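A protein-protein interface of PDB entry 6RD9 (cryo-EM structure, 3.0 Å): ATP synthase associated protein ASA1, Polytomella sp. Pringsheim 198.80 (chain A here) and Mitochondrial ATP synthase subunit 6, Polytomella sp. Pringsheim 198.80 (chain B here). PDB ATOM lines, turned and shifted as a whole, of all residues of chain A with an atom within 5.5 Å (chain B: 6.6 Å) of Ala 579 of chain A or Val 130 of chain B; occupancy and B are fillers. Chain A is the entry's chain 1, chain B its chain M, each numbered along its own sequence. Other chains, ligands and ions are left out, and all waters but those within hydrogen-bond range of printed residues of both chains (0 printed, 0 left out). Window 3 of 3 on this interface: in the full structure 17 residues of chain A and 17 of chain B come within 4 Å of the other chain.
O of Met 574 of chain A touches CG of Lys 125 of chain B (3.5 Å).
Met 574 of chain A touches Pro 126 of chain B (CB to CD, 3.9 Å).
Val 138 of chain B touches Met 574 of chain A (CG1 to SD, 3.7 Å).
Ala 576 of chain A touches Val 130 of chain B (CB to CB, 3.7 Å).
Ala 579 of chain A touches Val 130 of chain B.
Printed residues of chain B within 4 Å of Ala 579 of chain A: Val 130.
Val 130 of chain B touches just these residues of chain A: Ala 576 (3.7 Å) and Ala 579 (3.8 Å).
Of the printed residues of chain A, Val 138 of chain B touches Met 574 (3.7 Å).
Printed residues of chain A within 4 Å of Asp 132 of chain B: Gln 582 (3.4 Å).
Printed residues of chain B within 4 Å of Ala 576 of chain A: Val 130 (3.7 Å).
Printed residues of chain B within 4 Å of Met 574 of chain A: Lys 125, Pro 126 and Val 138.
Printed residues of chain B within 4 Å of Gln 582 of chain A: Asp 132.
Pro 129 of chain B touches none of the printed residues of chain A.
The nearest residue of chain A that does not touch Val 130 of chain B is Met 574 of chain A (4.2 Å).
The side-chain carboxylate (OD2) of Asp 132 of chain B is in hydrogen-bond range of the side-chain amide nitrogen (NE2) of Gln 582 of chain A.
The backbone NH (N) of Ala 576 of chain A sits at hydrogen-bond distance from the backbone carbonyl oxygen (O) of Leu 571 of chain A, at 2.8 Å.
Printed residues of chain B that touch a printed residue of chain A: Lys 125, Pro 126, Val 130, Asp 132 and Val 138.
Hydrophobic or aromatic side chains of chain B that line the printed part of chain A: Pro 126, Val 130 and Val 138.
Along chain B the printed residues that touch a printed residue of chain A span positions 125 to 138.
Of the 11 printed residues of chain A, 4 touch a printed residue of chain B.
Printed residues of chain A that touch a printed residue of chain B: Met 574, Ala 576, Ala 579 and Gln 582.
Among the printed residues, 6 pairs touch across the chains.
Among the printed residues, no Asp or Glu carboxylate lies within 4 Å of a Lys or Arg side-chain nitrogen of the other chain.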
ATOM      1  N   LEU A 571     -14.166 -15.598  28.594  1.00  0.00           N
ATOM      2  CA  LEU A 571     -13.417 -14.820  27.621  1.00  0.00           C
ATOM      3  C   LEU A 571     -12.362 -13.935  28.253  1.00  0.00           C
ATOM      4  O   LEU A 571     -11.435 -13.530  27.564  1.00  0.00           O
ATOM      5  CB  LEU A 571     -14.351 -13.947  26.804  1.00  0.00           C
ATOM      6  CG  LEU A 571     -15.345 -14.680  25.938  1.00  0.00           C
ATOM      7  CD1 LEU A 571     -16.311 -13.716  25.398  1.00  0.00           C
ATOM      8  CD2 LEU A 571     -14.647 -15.379  24.836  1.00  0.00           C
ATOM      9  N   MET A 574      -9.336 -16.559  29.023  1.00  0.00           N
ATOM     10  CA  MET A 574      -8.561 -16.900  27.851  1.00  0.00           C
ATOM     11  C   MET A 574      -8.132 -15.684  27.065  1.00  0.00           C
ATOM     12  O   MET A 574      -7.777 -15.816  25.893  1.00  0.00           O
ATOM     13  CB  MET A 574      -9.333 -17.872  26.968  1.00  0.00           C
ATOM     14  CG  MET A 574     -10.650 -17.435  26.535  1.00  0.00           C
ATOM     15  SD  MET A 574     -11.553 -18.785  25.810  1.00  0.00           S
ATOM     16  CE  MET A 574     -11.205 -20.087  26.955  1.00  0.00           C
ATOM     17  N   ALA A 576      -9.471 -13.298  25.521  1.00  0.00           N
ATOM     18  CA  ALA A 576     -10.132 -12.989  24.262  1.00  0.00           C
ATOM     19  C   ALA A 576     -10.705 -11.591  24.350  1.00  0.00           C
ATOM     20  O   ALA A 576     -11.885 -11.390  24.615  1.00  0.00           O
ATOM     21  CB  ALA A 576     -11.223 -13.999  23.968  1.00  0.00           C
ATOM     22  N   GLU A 577      -9.858 -10.600  24.111  1.00  0.00           N
ATOM     23  CA  GLU A 577     -10.339  -9.234  24.246  1.00  0.00           C
ATOM     24  C   GLU A 577     -11.144  -8.795  23.038  1.00  0.00           C
ATOM     25  O   GLU A 577     -11.956  -7.876  23.143  1.00  0.00           O
ATOM     26  CB  GLU A 577      -9.177  -8.286  24.509  1.00  0.00           C
ATOM     27  CG  GLU A 577      -8.750  -8.286  25.965  1.00  0.00           C
ATOM     28  CD  GLU A 577      -9.931  -8.144  26.932  1.00  0.00           C
ATOM     29  OE1 GLU A 577     -10.523  -7.045  26.999  1.00  0.00           O
ATOM     30  OE2 GLU A 577     -10.269  -9.133  27.628  1.00  0.00           O
ATOM     31  N   ASP A 578     -10.934  -9.420  21.887  1.00  0.00           N
ATOM     32  CA  ASP A 578     -11.718  -9.099  20.706  1.00  0.00           C
ATOM     33  C   ASP A 578     -12.966  -9.943  20.577  1.00  0.00           C
ATOM     34  O   ASP A 578     -13.845  -9.594  19.793  1.00  0.00           O
ATOM     35  CB  ASP A 578     -10.886  -9.270  19.447  1.00  0.00           C
ATOM     36  CG  ASP A 578     -10.112  -8.032  19.097  1.00  0.00           C
ATOM     37  OD1 ASP A 578      -9.025  -8.161  18.493  1.00  0.00           O
ATOM     38  OD2 ASP A 578     -10.584  -6.927  19.431  1.00  0.00           O
ATOM     39  N   ALA A 579     -13.039 -11.073  21.266  1.00  0.00           N
ATOM     40  CA  ALA A 579     -14.289 -11.807  21.354  1.00  0.00           C
ATOM     41  C   ALA A 579     -15.127 -11.345  22.521  1.00  0.00           C
ATOM     42  O   ALA A 579     -16.296 -11.713  22.606  1.00  0.00           O
ATOM     43  CB  ALA A 579     -14.035 -13.299  21.482  1.00  0.00           C
ATOM     44  N   LYS A 580     -14.537 -10.586  23.436  1.00  0.00           N
ATOM     45  CA  LYS A 580     -15.290  -9.875  24.453  1.00  0.00           C
ATOM     46  C   LYS A 580     -15.968  -8.648  23.879  1.00  0.00           C
ATOM     47  O   LYS A 580     -17.082  -8.325  24.278  1.00  0.00           O
ATOM     48  CB  LYS A 580     -14.359  -9.490  25.593  1.00  0.00           C
ATOM     49  CG  LYS A 580     -14.977  -8.766  26.738  1.00  0.00           C
ATOM     50  CD  LYS A 580     -15.706  -9.694  27.645  1.00  0.00           C
ATOM     51  CE  LYS A 580     -15.965  -9.029  28.969  1.00  0.00           C
ATOM     52  NZ  LYS A 580     -14.706  -8.702  29.665  1.00  0.00           N
ATOM     53  N   GLU A 581     -15.331  -7.963  22.934  1.00  0.00           N
ATOM     54  CA  GLU A 581     -15.978  -6.840  22.273  1.00  0.00           C
ATOM     55  C   GLU A 581     -17.046  -7.296  21.305  1.00  0.00           C
ATOM     56  O   GLU A 581     -18.017  -6.583  21.089  1.00  0.00           O
ATOM     57  CB  GLU A 581     -14.959  -5.999  21.538  1.00  0.00           C
ATOM     58  CG  GLU A 581     -13.988  -5.302  22.429  1.00  0.00           C
ATOM     59  CD  GLU A 581     -13.191  -4.255  21.689  1.00  0.00           C
ATOM     60  OE1 GLU A 581     -13.801  -3.439  20.966  1.00  0.00           O
ATOM     61  OE2 GLU A 581     -11.948  -4.259  21.818  1.00  0.00           O
ATOM     62  N   GLN A 582     -16.882  -8.455  20.700  1.00  0.00           N
ATOM     63  CA  GLN A 582     -17.936  -9.028  19.885  1.00  0.00           C
ATOM     64  C   GLN A 582     -19.078  -9.541  20.728  1.00  0.00           C
ATOM     65  O   GLN A 582     -20.217  -9.532  20.279  1.00  0.00           O
ATOM     66  CB  GLN A 582     -17.379 -10.168  19.051  1.00  0.00           C
ATOM     67  CG  GLN A 582     -18.295 -10.663  17.976  1.00  0.00           C
ATOM     68  CD  GLN A 582     -18.132 -12.128  17.705  1.00  0.00           C
ATOM     69  OE1 GLN A 582     -17.133 -12.729  18.069  1.00  0.00           O
ATOM     70  NE2 GLN A 582     -19.121 -12.716  17.073  1.00  0.00           N
ATOM     71  N   TRP A 583     -18.795 -10.007  21.939  1.00  0.00           N
ATOM     72  CA  TRP A 583     -19.856 -10.491  22.808  1.00  0.00           C
ATOM     73  C   TRP A 583     -20.738  -9.354  23.259  1.00  0.00           C
ATOM     74  O   TRP A 583     -21.960  -9.487  23.283  1.00  0.00           O
ATOM     75  CB  TRP A 583     -19.260 -11.214  24.006  1.00  0.00           C
ATOM     76  CG  TRP A 583     -20.196 -11.439  25.138  1.00  0.00           C
ATOM     77  CD1 TRP A 583     -21.105 -12.429  25.259  1.00  0.00           C
ATOM     78  CD2 TRP A 583     -20.293 -10.667  26.322  1.00  0.00           C
ATOM     79  NE1 TRP A 583     -21.779 -12.311  26.425  1.00  0.00           N
ATOM     80  CE2 TRP A 583     -21.295 -11.228  27.098  1.00  0.00           C
ATOM     81  CE3 TRP A 583     -19.642  -9.533  26.790  1.00  0.00           C
ATOM     82  CZ2 TRP A 583     -21.648 -10.714  28.317  1.00  0.00           C
ATOM     83  CZ3 TRP A 583     -19.993  -9.036  27.987  1.00  0.00           C
ATOM     84  CH2 TRP A 583     -20.977  -9.624  28.747  1.00  0.00           C
ATOM     85  N   GLY A 584     -20.142  -8.217  23.588  1.00  0.00           N
ATOM     86  CA  GLY A 584     -20.933  -7.068  23.950  1.00  0.00           C
ATOM     87  C   GLY A 584     -21.660  -6.464  22.779  1.00  0.00           C
ATOM     88  O   GLY A 584     -22.775  -5.985  22.928  1.00  0.00           O
ATOM     89  N   LYS B 125      -6.394 -20.642  28.114  1.00  0.00           N
ATOM     90  CA  LYS B 125      -6.302 -19.969  26.837  1.00  0.00           C
ATOM     91  C   LYS B 125      -5.904 -20.956  25.752  1.00  0.00           C
ATOM     92  O   LYS B 125      -4.933 -21.693  25.926  1.00  0.00           O
ATOM     93  CB  LYS B 125      -5.274 -18.869  26.940  1.00  0.00           C
ATOM     94  CG  LYS B 125      -5.103 -18.036  25.724  1.00  0.00           C
ATOM     95  CD  LYS B 125      -4.201 -16.882  26.065  1.00  0.00           C
ATOM     96  CE  LYS B 125      -4.264 -15.810  25.012  1.00  0.00           C
ATOM     97  NZ  LYS B 125      -3.556 -14.574  25.442  1.00  0.00           N
ATOM     98  N   PRO B 126      -6.622 -21.014  24.641  1.00  0.00           N
ATOM     99  CA  PRO B 126      -6.214 -21.882  23.541  1.00  0.00           C
ATOM    100  C   PRO B 126      -5.014 -21.295  22.814  1.00  0.00           C
ATOM    101  O   PRO B 126      -4.635 -20.144  23.010  1.00  0.00           O
ATOM    102  CB  PRO B 126      -7.447 -21.909  22.638  1.00  0.00           C
ATOM    103  CG  PRO B 126      -8.520 -21.297  23.413  1.00  0.00           C
ATOM    104  CD  PRO B 126      -7.891 -20.352  24.340  1.00  0.00           C
ATOM    105  N   ASP B 128      -5.025 -20.986  19.548  1.00  0.00           N
ATOM    106  CA  ASP B 128      -5.632 -20.222  18.484  1.00  0.00           C
ATOM    107  C   ASP B 128      -6.175 -18.900  19.014  1.00  0.00           C
ATOM    108  O   ASP B 128      -6.402 -18.749  20.214  1.00  0.00           O
ATOM    109  CB  ASP B 128      -6.759 -21.039  17.878  1.00  0.00           C
ATOM    110  CG  ASP B 128      -6.264 -22.282  17.211  1.00  0.00           C
ATOM    111  OD1 ASP B 128      -5.187 -22.237  16.585  1.00  0.00           O
ATOM    112  OD2 ASP B 128      -6.923 -23.325  17.356  1.00  0.00           O
ATOM    113  N   PRO B 129      -6.374 -17.913  18.148  1.00  0.00           N
ATOM    114  CA  PRO B 129      -7.142 -16.737  18.558  1.00  0.00           C
ATOM    115  C   PRO B 129      -8.613 -17.083  18.651  1.00  0.00           C
ATOM    116  O   PRO B 129      -9.130 -17.876  17.864  1.00  0.00           O
ATOM    117  CB  PRO B 129      -6.883 -15.732  17.433  1.00  0.00           C
ATOM    118  CG  PRO B 129      -5.690 -16.236  16.734  1.00  0.00           C
ATOM    119  CD  PRO B 129      -5.741 -17.711  16.839  1.00  0.00           C
ATOM    120  N   VAL B 130      -9.294 -16.489  19.621  1.00  0.00           N
ATOM    121  CA  VAL B 130     -10.712 -16.767  19.805  1.00  0.00           C
ATOM    122  C   VAL B 130     -11.485 -15.850  18.869  1.00  0.00           C
ATOM    123  O   VAL B 130     -11.492 -14.631  19.041  1.00  0.00           O
ATOM    124  CB  VAL B 130     -11.153 -16.578  21.258  1.00  0.00           C
ATOM    125  CG1 VAL B 130     -12.539 -17.119  21.443  1.00  0.00           C
ATOM    126  CG2 VAL B 130     -10.200 -17.239  22.199  1.00  0.00           C
ATOM    127  N   ASN B 131     -12.116 -16.436  17.863  1.00  0.00           N
ATOM    128  CA  ASN B 131     -12.959 -15.731  16.915  1.00  0.00           C
ATOM    129  C   ASN B 131     -14.143 -16.647  16.650  1.00  0.00           C
ATOM    130  O   ASN B 131     -14.364 -17.602  17.395  1.00  0.00           O
ATOM    131  CB  ASN B 131     -12.146 -15.342  15.678  1.00  0.00           C
ATOM    132  CG  ASN B 131     -11.305 -16.475  15.148  1.00  0.00           C
ATOM    133  OD1 ASN B 131     -11.441 -17.618  15.557  1.00  0.00           O
ATOM    134  ND2 ASN B 131     -10.394 -16.148  14.251  1.00  0.00           N
ATOM    135  N   ASP B 132     -14.909 -16.388  15.591  1.00  0.00           N
ATOM    136  CA  ASP B 132     -16.077 -17.219  15.303  1.00  0.00           C
ATOM    137  C   ASP B 132     -15.722 -18.632  14.881  1.00  0.00           C
ATOM    138  O   ASP B 132     -16.605 -19.489  14.842  1.00  0.00           O
ATOM    139  CB  ASP B 132     -16.931 -16.607  14.203  1.00  0.00           C
ATOM    140  CG  ASP B 132     -17.645 -15.364  14.638  1.00  0.00           C
ATOM    141  OD1 ASP B 132     -17.113 -14.263  14.399  1.00  0.00           O
ATOM    142  OD2 ASP B 132     -18.752 -15.482  15.197  1.00  0.00           O
ATOM    143  N   ARG B 133     -14.474 -18.886  14.522  1.00  0.00           N
ATOM    144  CA  ARG B 133     -14.038 -20.249  14.283  1.00  0.00           C
ATOM    145  C   ARG B 133     -13.914 -21.006  15.592  1.00  0.00           C
ATOM    146  O   ARG B 133     -14.371 -22.144  15.704  1.00  0.00           O
ATOM    147  CB  ARG B 133     -12.706 -20.230  13.544  1.00  0.00           C
ATOM    148  CG  ARG B 133     -12.140 -21.584  13.232  1.00  0.00           C
ATOM    149  CD  ARG B 133     -12.782 -22.198  12.025  1.00  0.00           C
ATOM    150  NE  ARG B 133     -12.322 -23.563  11.859  1.00  0.00           N
ATOM    151  CZ  ARG B 133     -12.981 -24.614  12.312  1.00  0.00           C
ATOM    152  NH1 ARG B 133     -14.128 -24.440  12.932  1.00  0.00           N
ATOM    153  NH2 ARG B 133     -12.506 -25.830  12.140  1.00  0.00           N
ATOM    154  N   LEU B 134     -13.337 -20.372  16.597  1.00  0.00           N
ATOM    155  CA  LEU B 134     -13.038 -21.019  17.857  1.00  0.00           C
ATOM    156  C   LEU B 134     -14.167 -20.899  18.864  1.00  0.00           C
ATOM    157  O   LEU B 134     -14.063 -21.444  19.959  1.00  0.00           O
ATOM    158  CB  LEU B 134     -11.767 -20.417  18.432  1.00  0.00           C
ATOM    159  CG  LEU B 134     -10.909 -21.317  19.293  1.00  0.00           C
ATOM    160  CD1 LEU B 134     -10.372 -22.389  18.432  1.00  0.00           C
ATOM    161  CD2 LEU B 134      -9.806 -20.543  19.916  1.00  0.00           C
ATOM    162  N   LEU B 135     -15.245 -20.208  18.525  1.00  0.00           N
ATOM    163  CA  LEU B 135     -16.308 -19.987  19.497  1.00  0.00           C
ATOM    164  C   LEU B 135     -17.102 -21.229  19.862  1.00  0.00           C
ATOM    165  O   LEU B 135     -17.494 -21.327  21.033  1.00  0.00           O
ATOM    166  CB  LEU B 135     -17.255 -18.887  19.020  1.00  0.00           C
ATOM    167  CG  LEU B 135     -17.000 -17.471  19.491  1.00  0.00           C
ATOM    168  CD1 LEU B 135     -18.160 -16.650  19.055  1.00  0.00           C
ATOM    169  CD2 LEU B 135     -16.809 -17.416  20.973  1.00  0.00           C
ATOM    170  N   VAL B 138     -14.878 -23.009  22.373  1.00  0.00           N
ATOM    171  CA  VAL B 138     -14.856 -22.346  23.669  1.00  0.00           C
ATOM    172  C   VAL B 138     -16.155 -22.587  24.425  1.00  0.00           C
ATOM    173  O   VAL B 138     -16.151 -22.783  25.640  1.00  0.00           O
ATOM    174  CB  VAL B 138     -14.565 -20.858  23.444  1.00  0.00           C
ATOM    175  CG1 VAL B 138     -14.815 -20.056  24.655  1.00  0.00           C
ATOM    176  CG2 VAL B 138     -13.145 -20.698  23.041  1.00  0.00           C
